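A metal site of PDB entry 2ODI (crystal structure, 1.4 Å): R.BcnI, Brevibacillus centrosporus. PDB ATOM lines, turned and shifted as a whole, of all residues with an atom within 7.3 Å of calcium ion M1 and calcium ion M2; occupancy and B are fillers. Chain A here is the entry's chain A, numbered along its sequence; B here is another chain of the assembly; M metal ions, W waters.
Water W2 lies within hydrogen-bond range of OP2 of DG 6 of chain B, the side-chain amino group (NZ) of Lys 62 and OP2 of DC 5 of chain B. Water W4 bridges OE2 of Glu 41 and O3' of DC 4 of chain B. Water W3 lies within hydrogen-bond range of the side-chain carboxylate (OE1) of Glu 60 and the side-chain amino group (NZ) of Lys 152.
Four residues have an atom within 4 Å of calcium ion M2: Asn 49, Asp 55, DC 4 of chain B and DC 5 of chain B.
Calcium ion M1 is bound by OD2 of Asp 55, at 2.1 Å. Calcium ion M1 is bound by OP1 of DC 5 of chain B (2.3 Å). Calcium ion M1 is bound by OE2 of Glu 60, at 2.3 Å. Calcium ion M1 is bound by water W1, at 2.4 Å. O of Leu 61 is bound to calcium ion M1 (2.4 Å). Water W2 binds calcium ion M1 (2.4 Å). Calcium ion M1 has six donor atoms within binding distance.
Of the 23 residues printed, 4 come within 4 Å of calcium ion M1.
Calcium ion M2 is bound by water W3 (2.2 Å), water W4 (2.2 Å), the side-chain carboxylate (OD1) of Asp 55 (2.4 Å), the side-chain amide oxygen (OD1) of Asn 49 (2.4 Å) and OP1 of DC 5 of chain B (2.6 Å). Calcium ion M2 has five donor atoms within binding distance. Slightly farther from calcium ion M2 lies O3' of DC 4 of chain B (2.9 Å).
The side-chain amino group of Lys 62 is in salt-bridge range of OP2 of DC 5 of chain B (3.99 Å). The backbone carbonyl oxygen (O) of Glu 60 sits at hydrogen-bond distance from the backbone NH (N) of Val 157. NZ of Lys 152 sits close to OD1 of Asn 49, at 3.2 Å. The side-chain carboxylate (OE2) of Glu 60 lies close to the side-chain amino group (NZ) of Lys 62, at 3.1 Å.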
ATOM      1  N   GLY A  37      -1.800 -18.314  23.614  1.00  0.00           N
ATOM      2  CA  GLY A  37      -2.190 -16.916  23.409  1.00  0.00           C
ATOM      3  C   GLY A  37      -3.357 -16.753  22.467  1.00  0.00           C
ATOM      4  O   GLY A  37      -4.186 -15.884  22.660  1.00  0.00           O
ATOM      5  N   GLU A  41      -6.894 -15.066  23.509  1.00  0.00           N
ATOM      6  CA  GLU A  41      -7.473 -13.993  22.686  1.00  0.00           C
ATOM      7  C   GLU A  41      -8.918 -14.283  22.317  1.00  0.00           C
ATOM      8  O   GLU A  41      -9.778 -13.387  22.380  1.00  0.00           O
ATOM      9  CB  GLU A  41      -6.655 -13.771  21.411  1.00  0.00           C
ATOM     10  CG  GLU A  41      -5.379 -13.027  21.663  1.00  0.00           C
ATOM     11  CD  GLU A  41      -4.544 -12.832  20.417  1.00  0.00           C
ATOM     12  OE1 GLU A  41      -4.600 -13.705  19.506  1.00  0.00           O
ATOM     13  OE2 GLU A  41      -3.817 -11.819  20.343  1.00  0.00           O
ATOM     14  N   VAL A  46     -10.699 -10.951  20.957  1.00  0.00           N
ATOM     15  CA  VAL A  46      -9.665 -10.178  20.271  1.00  0.00           C
ATOM     16  C   VAL A  46      -9.501 -10.744  18.856  1.00  0.00           C
ATOM     17  O   VAL A  46      -8.975 -11.845  18.684  1.00  0.00           O
ATOM     18  CB  VAL A  46      -8.338 -10.195  21.063  1.00  0.00           C
ATOM     19  CG1 VAL A  46      -7.198  -9.545  20.278  1.00  0.00           C
ATOM     20  CG2 VAL A  46      -8.518  -9.508  22.416  1.00  0.00           C
ATOM     21  N   GLU A  48      -8.164  -9.208  15.909  1.00  0.00           N
ATOM     22  CA  GLU A  48      -6.953  -8.867  15.162  1.00  0.00           C
ATOM     23  C   GLU A  48      -6.077  -7.987  16.035  1.00  0.00           C
ATOM     24  O   GLU A  48      -6.544  -7.404  17.016  1.00  0.00           O
ATOM     25  CB  GLU A  48      -7.286  -8.157  13.842  1.00  0.00           C
ATOM     26  CG  GLU A  48      -8.004  -6.808  13.981  1.00  0.00           C
ATOM     27  CD  GLU A  48      -8.406  -6.217  12.638  1.00  0.00           C
ATOM     28  OE1 GLU A  48      -9.613  -5.980  12.444  1.00  0.00           O
ATOM     29  OE2 GLU A  48      -7.519  -6.021  11.777  1.00  0.00           O
ATOM     30  N   ASN A  49      -4.790  -7.897  15.675  1.00  0.00           N
ATOM     31  CA  ASN A  49      -3.894  -6.955  16.320  1.00  0.00           C
ATOM     32  C   ASN A  49      -4.296  -5.522  15.977  1.00  0.00           C
ATOM     33  O   ASN A  49      -4.696  -5.233  14.846  1.00  0.00           O
ATOM     34  CB  ASN A  49      -2.452  -7.190  15.884  1.00  0.00           C
ATOM     35  CG  ASN A  49      -1.475  -6.301  16.631  1.00  0.00           C
ATOM     36  OD1 ASN A  49      -1.395  -6.367  17.863  1.00  0.00           O
ATOM     37  ND2 ASN A  49      -0.751  -5.462  15.913  1.00  0.00           N
ATOM     38  N   ASN A  50      -4.189  -4.647  16.970  1.00  0.00           N
ATOM     39  CA  ASN A  50      -4.344  -3.216  16.758  1.00  0.00           C
ATOM     40  C   ASN A  50      -2.970  -2.563  16.868  1.00  0.00           C
ATOM     41  O   ASN A  50      -2.268  -2.778  17.851  1.00  0.00           O
ATOM     42  CB  ASN A  50      -5.313  -2.620  17.778  1.00  0.00           C
ATOM     43  CG  ASN A  50      -5.663  -1.177  17.473  1.00  0.00           C
ATOM     44  OD1 ASN A  50      -4.881  -0.270  17.763  1.00  0.00           O
ATOM     45  ND2 ASN A  50      -6.849  -0.956  16.908  1.00  0.00           N
ATOM     46  N   ILE A  51      -2.607  -1.770  15.856  1.00  0.00           N
ATOM     47  CA  ILE A  51      -1.281  -1.146  15.810  1.00  0.00           C
ATOM     48  C   ILE A  51      -1.080  -0.094  16.910  1.00  0.00           C
ATOM     49  O   ILE A  51       0.037   0.140  17.364  1.00  0.00           O
ATOM     50  CB  ILE A  51      -0.944  -0.554  14.410  1.00  0.00           C
ATOM     51  CG1 ILE A  51      -2.028   0.419  13.923  1.00  0.00           C
ATOM     52  CG2 ILE A  51      -0.715  -1.687  13.402  1.00  0.00           C
ATOM     53  CD1 ILE A  51      -1.737   1.078  12.565  1.00  0.00           C
ATOM     54  N   LEU A  53      -2.941   0.181  20.095  1.00  0.00           N
ATOM     55  CA  LEU A  53      -3.229  -0.102  21.501  1.00  0.00           C
ATOM     56  C   LEU A  53      -2.971  -1.553  21.903  1.00  0.00           C
ATOM     57  O   LEU A  53      -3.012  -2.445  21.062  1.00  0.00           O
ATOM     58  CB  LEU A  53      -4.692   0.231  21.771  1.00  0.00           C
ATOM     59  CG  LEU A  53      -5.186   1.646  21.448  1.00  0.00           C
ATOM     60  CD1 LEU A  53      -6.683   1.707  21.670  1.00  0.00           C
ATOM     61  CD2 LEU A  53      -4.441   2.685  22.302  1.00  0.00           C
ATOM     62  N   GLY A  54      -2.743  -1.758  23.202  1.00  0.00           N
ATOM     63  CA  GLY A  54      -2.793  -3.114  23.791  1.00  0.00           C
ATOM     64  C   GLY A  54      -4.102  -3.799  23.424  1.00  0.00           C
ATOM     65  O   GLY A  54      -5.114  -3.124  23.161  1.00  0.00           O
ATOM     66  N   ASP A  55      -4.105  -5.141  23.420  1.00  0.00           N
ATOM     67  CA  ASP A  55      -5.237  -5.940  22.906  1.00  0.00           C
ATOM     68  C   ASP A  55      -6.583  -5.564  23.507  1.00  0.00           C
ATOM     69  O   ASP A  55      -7.612  -5.703  22.837  1.00  0.00           O
ATOM     70  CB  ASP A  55      -5.045  -7.444  23.164  1.00  0.00           C
ATOM     71  CG  ASP A  55      -3.769  -7.988  22.592  1.00  0.00           C
ATOM     72  OD1 ASP A  55      -3.646  -8.088  21.348  1.00  0.00           O
ATOM     73  OD2 ASP A  55      -2.886  -8.313  23.391  1.00  0.00           O
ATOM     74  N   LEU A  56      -6.581  -5.146  24.767  1.00  0.00           N
ATOM     75  CA  LEU A  56      -7.829  -4.894  25.493  1.00  0.00           C
ATOM     76  C   LEU A  56      -8.163  -3.411  25.585  1.00  0.00           C
ATOM     77  O   LEU A  56      -9.198  -3.055  26.151  1.00  0.00           O
ATOM     78  CB  LEU A  56      -7.771  -5.514  26.894  1.00  0.00           C
ATOM     79  CG  LEU A  56      -7.449  -7.003  26.976  1.00  0.00           C
ATOM     80  CD1 LEU A  56      -7.372  -7.434  28.434  1.00  0.00           C
ATOM     81  CD2 LEU A  56      -8.480  -7.840  26.208  1.00  0.00           C
ATOM     82  N   PHE A  59      -5.126  -2.077  28.376  1.00  0.00           N
ATOM     83  CA  PHE A  59      -4.204  -3.131  28.760  1.00  0.00           C
ATOM     84  C   PHE A  59      -3.820  -3.987  27.576  1.00  0.00           C
ATOM     85  O   PHE A  59      -4.622  -4.229  26.688  1.00  0.00           O
ATOM     86  CB  PHE A  59      -4.846  -4.035  29.808  1.00  0.00           C
ATOM     87  CG  PHE A  59      -5.720  -3.311  30.793  1.00  0.00           C
ATOM     88  CD1 PHE A  59      -5.166  -2.466  31.733  1.00  0.00           C
ATOM     89  CD2 PHE A  59      -7.104  -3.473  30.749  1.00  0.00           C
ATOM     90  CE1 PHE A  59      -5.969  -1.783  32.637  1.00  0.00           C
ATOM     91  CE2 PHE A  59      -7.923  -2.787  31.652  1.00  0.00           C
ATOM     92  CZ  PHE A  59      -7.349  -1.948  32.602  1.00  0.00           C
ATOM     93  N   GLU A  60      -2.591  -4.468  27.618  1.00  0.00           N
ATOM     94  CA  GLU A  60      -2.104  -5.480  26.689  1.00  0.00           C
ATOM     95  C   GLU A  60      -2.293  -6.873  27.327  1.00  0.00           C
ATOM     96  O   GLU A  60      -1.957  -7.063  28.499  1.00  0.00           O
ATOM     97  CB  GLU A  60      -0.631  -5.201  26.367  1.00  0.00           C
ATOM     98  CG  GLU A  60       0.146  -6.341  25.698  1.00  0.00           C
ATOM     99  CD  GLU A  60      -0.327  -6.729  24.310  1.00  0.00           C
ATOM    100  OE1 GLU A  60      -1.036  -5.931  23.650  1.00  0.00           O
ATOM    101  OE2 GLU A  60       0.061  -7.829  23.862  1.00  0.00           O
ATOM    102  N   LEU A  61      -2.810  -7.829  26.564  1.00  0.00           N
ATOM    103  CA  LEU A  61      -3.095  -9.174  27.057  1.00  0.00           C
ATOM    104  C   LEU A  61      -1.983 -10.139  26.691  1.00  0.00           C
ATOM    105  O   LEU A  61      -1.582 -10.178  25.538  1.00  0.00           O
ATOM    106  CB  LEU A  61      -4.386  -9.660  26.398  1.00  0.00           C
ATOM    107  CG  LEU A  61      -4.884 -11.070  26.725  1.00  0.00           C
ATOM    108  CD1 LEU A  61      -5.317 -11.171  28.179  1.00  0.00           C
ATOM    109  CD2 LEU A  61      -6.020 -11.454  25.780  1.00  0.00           C
ATOM    110  N   LYS A  62      -1.509 -10.897  27.668  1.00  0.00           N
ATOM    111  CA  LYS A  62      -0.478 -11.941  27.472  1.00  0.00           C
ATOM    112  C   LYS A  62      -0.900 -13.202  28.186  1.00  0.00           C
ATOM    113  O   LYS A  62      -1.311 -13.151  29.350  1.00  0.00           O
ATOM    114  CB  LYS A  62       0.864 -11.528  28.084  1.00  0.00           C
ATOM    115  CG  LYS A  62       1.394 -10.190  27.673  1.00  0.00           C
ATOM    116  CD  LYS A  62       1.964 -10.218  26.296  1.00  0.00           C
ATOM    117  CE  LYS A  62       2.741  -8.942  26.013  1.00  0.00           C
ATOM    118  NZ  LYS A  62       2.886  -8.779  24.551  1.00  0.00           N
ATOM    119  N   GLY A  63      -0.737 -14.336  27.507  1.00  0.00           N
ATOM    120  CA  GLY A  63      -0.968 -15.649  28.105  1.00  0.00           C
ATOM    121  C   GLY A  63       0.336 -16.418  28.166  1.00  0.00           C
ATOM    122  O   GLY A  63       1.242 -16.177  27.363  1.00  0.00           O
ATOM    123  N   THR A  74       7.621 -12.562  26.203  1.00  0.00           N
ATOM    124  CA  THR A  74       7.834 -11.680  25.055  1.00  0.00           C
ATOM    125  C   THR A  74       6.914 -10.475  25.160  1.00  0.00           C
ATOM    126  O   THR A  74       5.687 -10.614  25.294  1.00  0.00           O
ATOM    127  CB  THR A  74       7.610 -12.412  23.736  1.00  0.00           C
ATOM    128  OG1 THR A  74       8.639 -13.404  23.587  1.00  0.00           O
ATOM    129  CG2 THR A  74       7.656 -11.441  22.524  1.00  0.00           C
ATOM    130  N   LEU A  75       7.517  -9.286  25.144  1.00  0.00           N
ATOM    131  CA  LEU A  75       6.781  -8.045  25.296  1.00  0.00           C
ATOM    132  C   LEU A  75       6.256  -7.515  23.958  1.00  0.00           C
ATOM    133  O   LEU A  75       5.067  -7.173  23.824  1.00  0.00           O
ATOM    134  CB  LEU A  75       7.647  -7.017  26.030  1.00  0.00           C
ATOM    135  CG  LEU A  75       8.022  -7.441  27.447  1.00  0.00           C
ATOM    136  CD1 LEU A  75       9.152  -6.593  27.994  1.00  0.00           C
ATOM    137  CD2 LEU A  75       6.826  -7.426  28.397  1.00  0.00           C
ATOM    138  N   LYS A 152       2.318   0.358  24.273  1.00  0.00           N
ATOM    139  CA  LYS A 152       1.349  -0.740  24.336  1.00  0.00           C
ATOM    140  C   LYS A 152       1.477  -1.595  25.586  1.00  0.00           C
ATOM    141  O   LYS A 152       0.494  -2.197  26.024  1.00  0.00           O
ATOM    142  CB  LYS A 152       1.427  -1.612  23.071  1.00  0.00           C
ATOM    143  CG  LYS A 152       0.720  -1.007  21.865  1.00  0.00           C
ATOM    144  CD  LYS A 152       0.751  -1.926  20.644  1.00  0.00           C
ATOM    145  CE  LYS A 152      -0.048  -3.214  20.885  1.00  0.00           C
ATOM    146  NZ  LYS A 152      -0.489  -3.849  19.606  1.00  0.00           N
ATOM    147  N   VAL A 157      -2.106  -7.294  31.276  1.00  0.00           N
ATOM    148  CA  VAL A 157      -2.860  -8.355  31.929  1.00  0.00           C
ATOM    149  C   VAL A 157      -2.178  -9.649  31.516  1.00  0.00           C
ATOM    150  O   VAL A 157      -2.156  -9.979  30.341  1.00  0.00           O
ATOM    151  CB  VAL A 157      -4.358  -8.339  31.524  1.00  0.00           C
ATOM    152  CG1 VAL A 157      -5.077  -9.581  32.057  1.00  0.00           C
ATOM    153  CG2 VAL A 157      -5.054  -7.073  32.042  1.00  0.00           C
ATOM    154  P    DC B   4       4.069  -6.379  17.691  1.00  0.00           P
ATOM    155  OP1  DC B   4       3.277  -5.442  18.538  1.00  0.00           O
ATOM    156  OP2  DC B   4       5.376  -6.877  18.182  1.00  0.00           O
ATOM    157  O5'  DC B   4       3.146  -7.637  17.355  1.00  0.00           O
ATOM    158  C5'  DC B   4       1.797  -7.474  16.929  1.00  0.00           C
ATOM    159  C4'  DC B   4       1.188  -8.826  16.660  1.00  0.00           C
ATOM    160  O4'  DC B   4       1.854  -9.484  15.561  1.00  0.00           O
ATOM    161  C3'  DC B   4       1.329  -9.810  17.799  1.00  0.00           C
ATOM    162  O3'  DC B   4       0.352  -9.538  18.798  1.00  0.00           O
ATOM    163  C2'  DC B   4       1.099 -11.136  17.099  1.00  0.00           C
ATOM    164  C1'  DC B   4       1.791 -10.896  15.756  1.00  0.00           C
ATOM    165  N1   DC B   4       3.158 -11.437  15.659  1.00  0.00           N
ATOM    166  C2   DC B   4       3.317 -12.818  15.536  1.00  0.00           C
ATOM    167  O2   DC B   4       2.312 -13.548  15.615  1.00  0.00           O
ATOM    168  N3   DC B   4       4.555 -13.340  15.348  1.00  0.00           N
ATOM    169  C4   DC B   4       5.613 -12.517  15.304  1.00  0.00           C
ATOM    170  N4   DC B   4       6.815 -13.066  15.076  1.00  0.00           N
ATOM    171  C5   DC B   4       5.488 -11.106  15.481  1.00  0.00           C
ATOM    172  C6   DC B   4       4.253 -10.616  15.654  1.00  0.00           C
ATOM    173  P    DC B   5       0.621  -9.984  20.314  1.00  0.00           P
ATOM    174  OP1  DC B   5      -0.590  -9.578  21.083  1.00  0.00           O
ATOM    175  OP2  DC B   5       1.953  -9.487  20.735  1.00  0.00           O
ATOM    176  O5'  DC B   5       0.696 -11.573  20.235  1.00  0.00           O
ATOM    177  C5'  DC B   5      -0.473 -12.341  19.987  1.00  0.00           C
ATOM    178  C4'  DC B   5      -0.147 -13.817  19.987  1.00  0.00           C
ATOM    179  O4'  DC B   5       0.657 -14.191  18.847  1.00  0.00           O
ATOM    180  C3'  DC B   5       0.683 -14.292  21.167  1.00  0.00           C
ATOM    181  O3'  DC B   5      -0.119 -14.357  22.352  1.00  0.00           O
ATOM    182  C2'  DC B   5       1.139 -15.655  20.668  1.00  0.00           C
ATOM    183  C1'  DC B   5       1.456 -15.338  19.199  1.00  0.00           C
ATOM    184  N1   DC B   5       2.873 -14.991  18.962  1.00  0.00           N
ATOM    185  C2   DC B   5       3.778 -16.026  18.742  1.00  0.00           C
ATOM    186  O2   DC B   5       3.375 -17.192  18.729  1.00  0.00           O
ATOM    187  N3   DC B   5       5.084 -15.717  18.549  1.00  0.00           N
ATOM    188  C4   DC B   5       5.486 -14.447  18.570  1.00  0.00           C
ATOM    189  N4   DC B   5       6.790 -14.193  18.381  1.00  0.00           N
ATOM    190  C5   DC B   5       4.575 -13.379  18.783  1.00  0.00           C
ATOM    191  C6   DC B   5       3.286 -13.690  18.977  1.00  0.00           C
ATOM    192  P    DG B   6       0.596 -14.479  23.794  1.00  0.00           P
ATOM    193  OP1  DG B   6      -0.485 -14.468  24.824  1.00  0.00           O
ATOM    194  OP2  DG B   6       1.700 -13.484  23.869  1.00  0.00           O
ATOM    195  O5'  DG B   6       1.215 -15.931  23.727  1.00  0.00           O
ATOM    196  C5'  DG B   6       2.420 -16.272  24.390  1.00  0.00           C
ATOM    197  C4'  DG B   6       3.065 -17.429  23.665  1.00  0.00           C
ATOM    198  O4'  DG B   6       3.753 -16.978  22.474  1.00  0.00           O
ATOM    199  C3'  DG B   6       4.119 -18.204  24.435  1.00  0.00           C
ATOM    200  O3'  DG B   6       3.454 -19.075  25.351  1.00  0.00           O
ATOM    201  C2'  DG B   6       4.779 -18.961  23.299  1.00  0.00           C
ATOM    202  C1'  DG B   6       4.788 -17.912  22.176  1.00  0.00           C
ATOM    203  N9   DG B   6       6.047 -17.185  22.077  1.00  0.00           N
ATOM    204  C8   DG B   6       6.293 -15.875  22.384  1.00  0.00           C
ATOM    205  N7   DG B   6       7.540 -15.541  22.247  1.00  0.00           N
ATOM    206  C5   DG B   6       8.163 -16.706  21.812  1.00  0.00           C
ATOM    207  C6   DG B   6       9.520 -16.976  21.530  1.00  0.00           C
ATOM    208  O6   DG B   6      10.503 -16.217  21.610  1.00  0.00           O
ATOM    209  N1   DG B   6       9.705 -18.296  21.114  1.00  0.00           N
ATOM    210  C2   DG B   6       8.707 -19.232  21.005  1.00  0.00           C
ATOM    211  N2   DG B   6       9.074 -20.450  20.579  1.00  0.00           N
ATOM    212  N3   DG B   6       7.439 -18.994  21.284  1.00  0.00           N
ATOM    213  C4   DG B   6       7.242 -17.722  21.687  1.00  0.00           C
HETATM  214 CA    CA M   1      -1.233  -9.650  23.263  1.00  0.00          CA
HETATM  215 CA    CA M   2      -1.926  -7.892  19.671  1.00  0.00          CA
HETATM  216  O   HOH W   1      -2.638 -11.502  22.858  1.00  0.00           O
HETATM  217  O   HOH W   2       0.809 -10.876  23.367  1.00  0.00           O
HETATM  218  O   HOH W   3      -0.956  -6.428  20.995  1.00  0.00           O
HETATM  219  O   HOH W   4      -3.135  -9.539  18.782  1.00  0.00           O
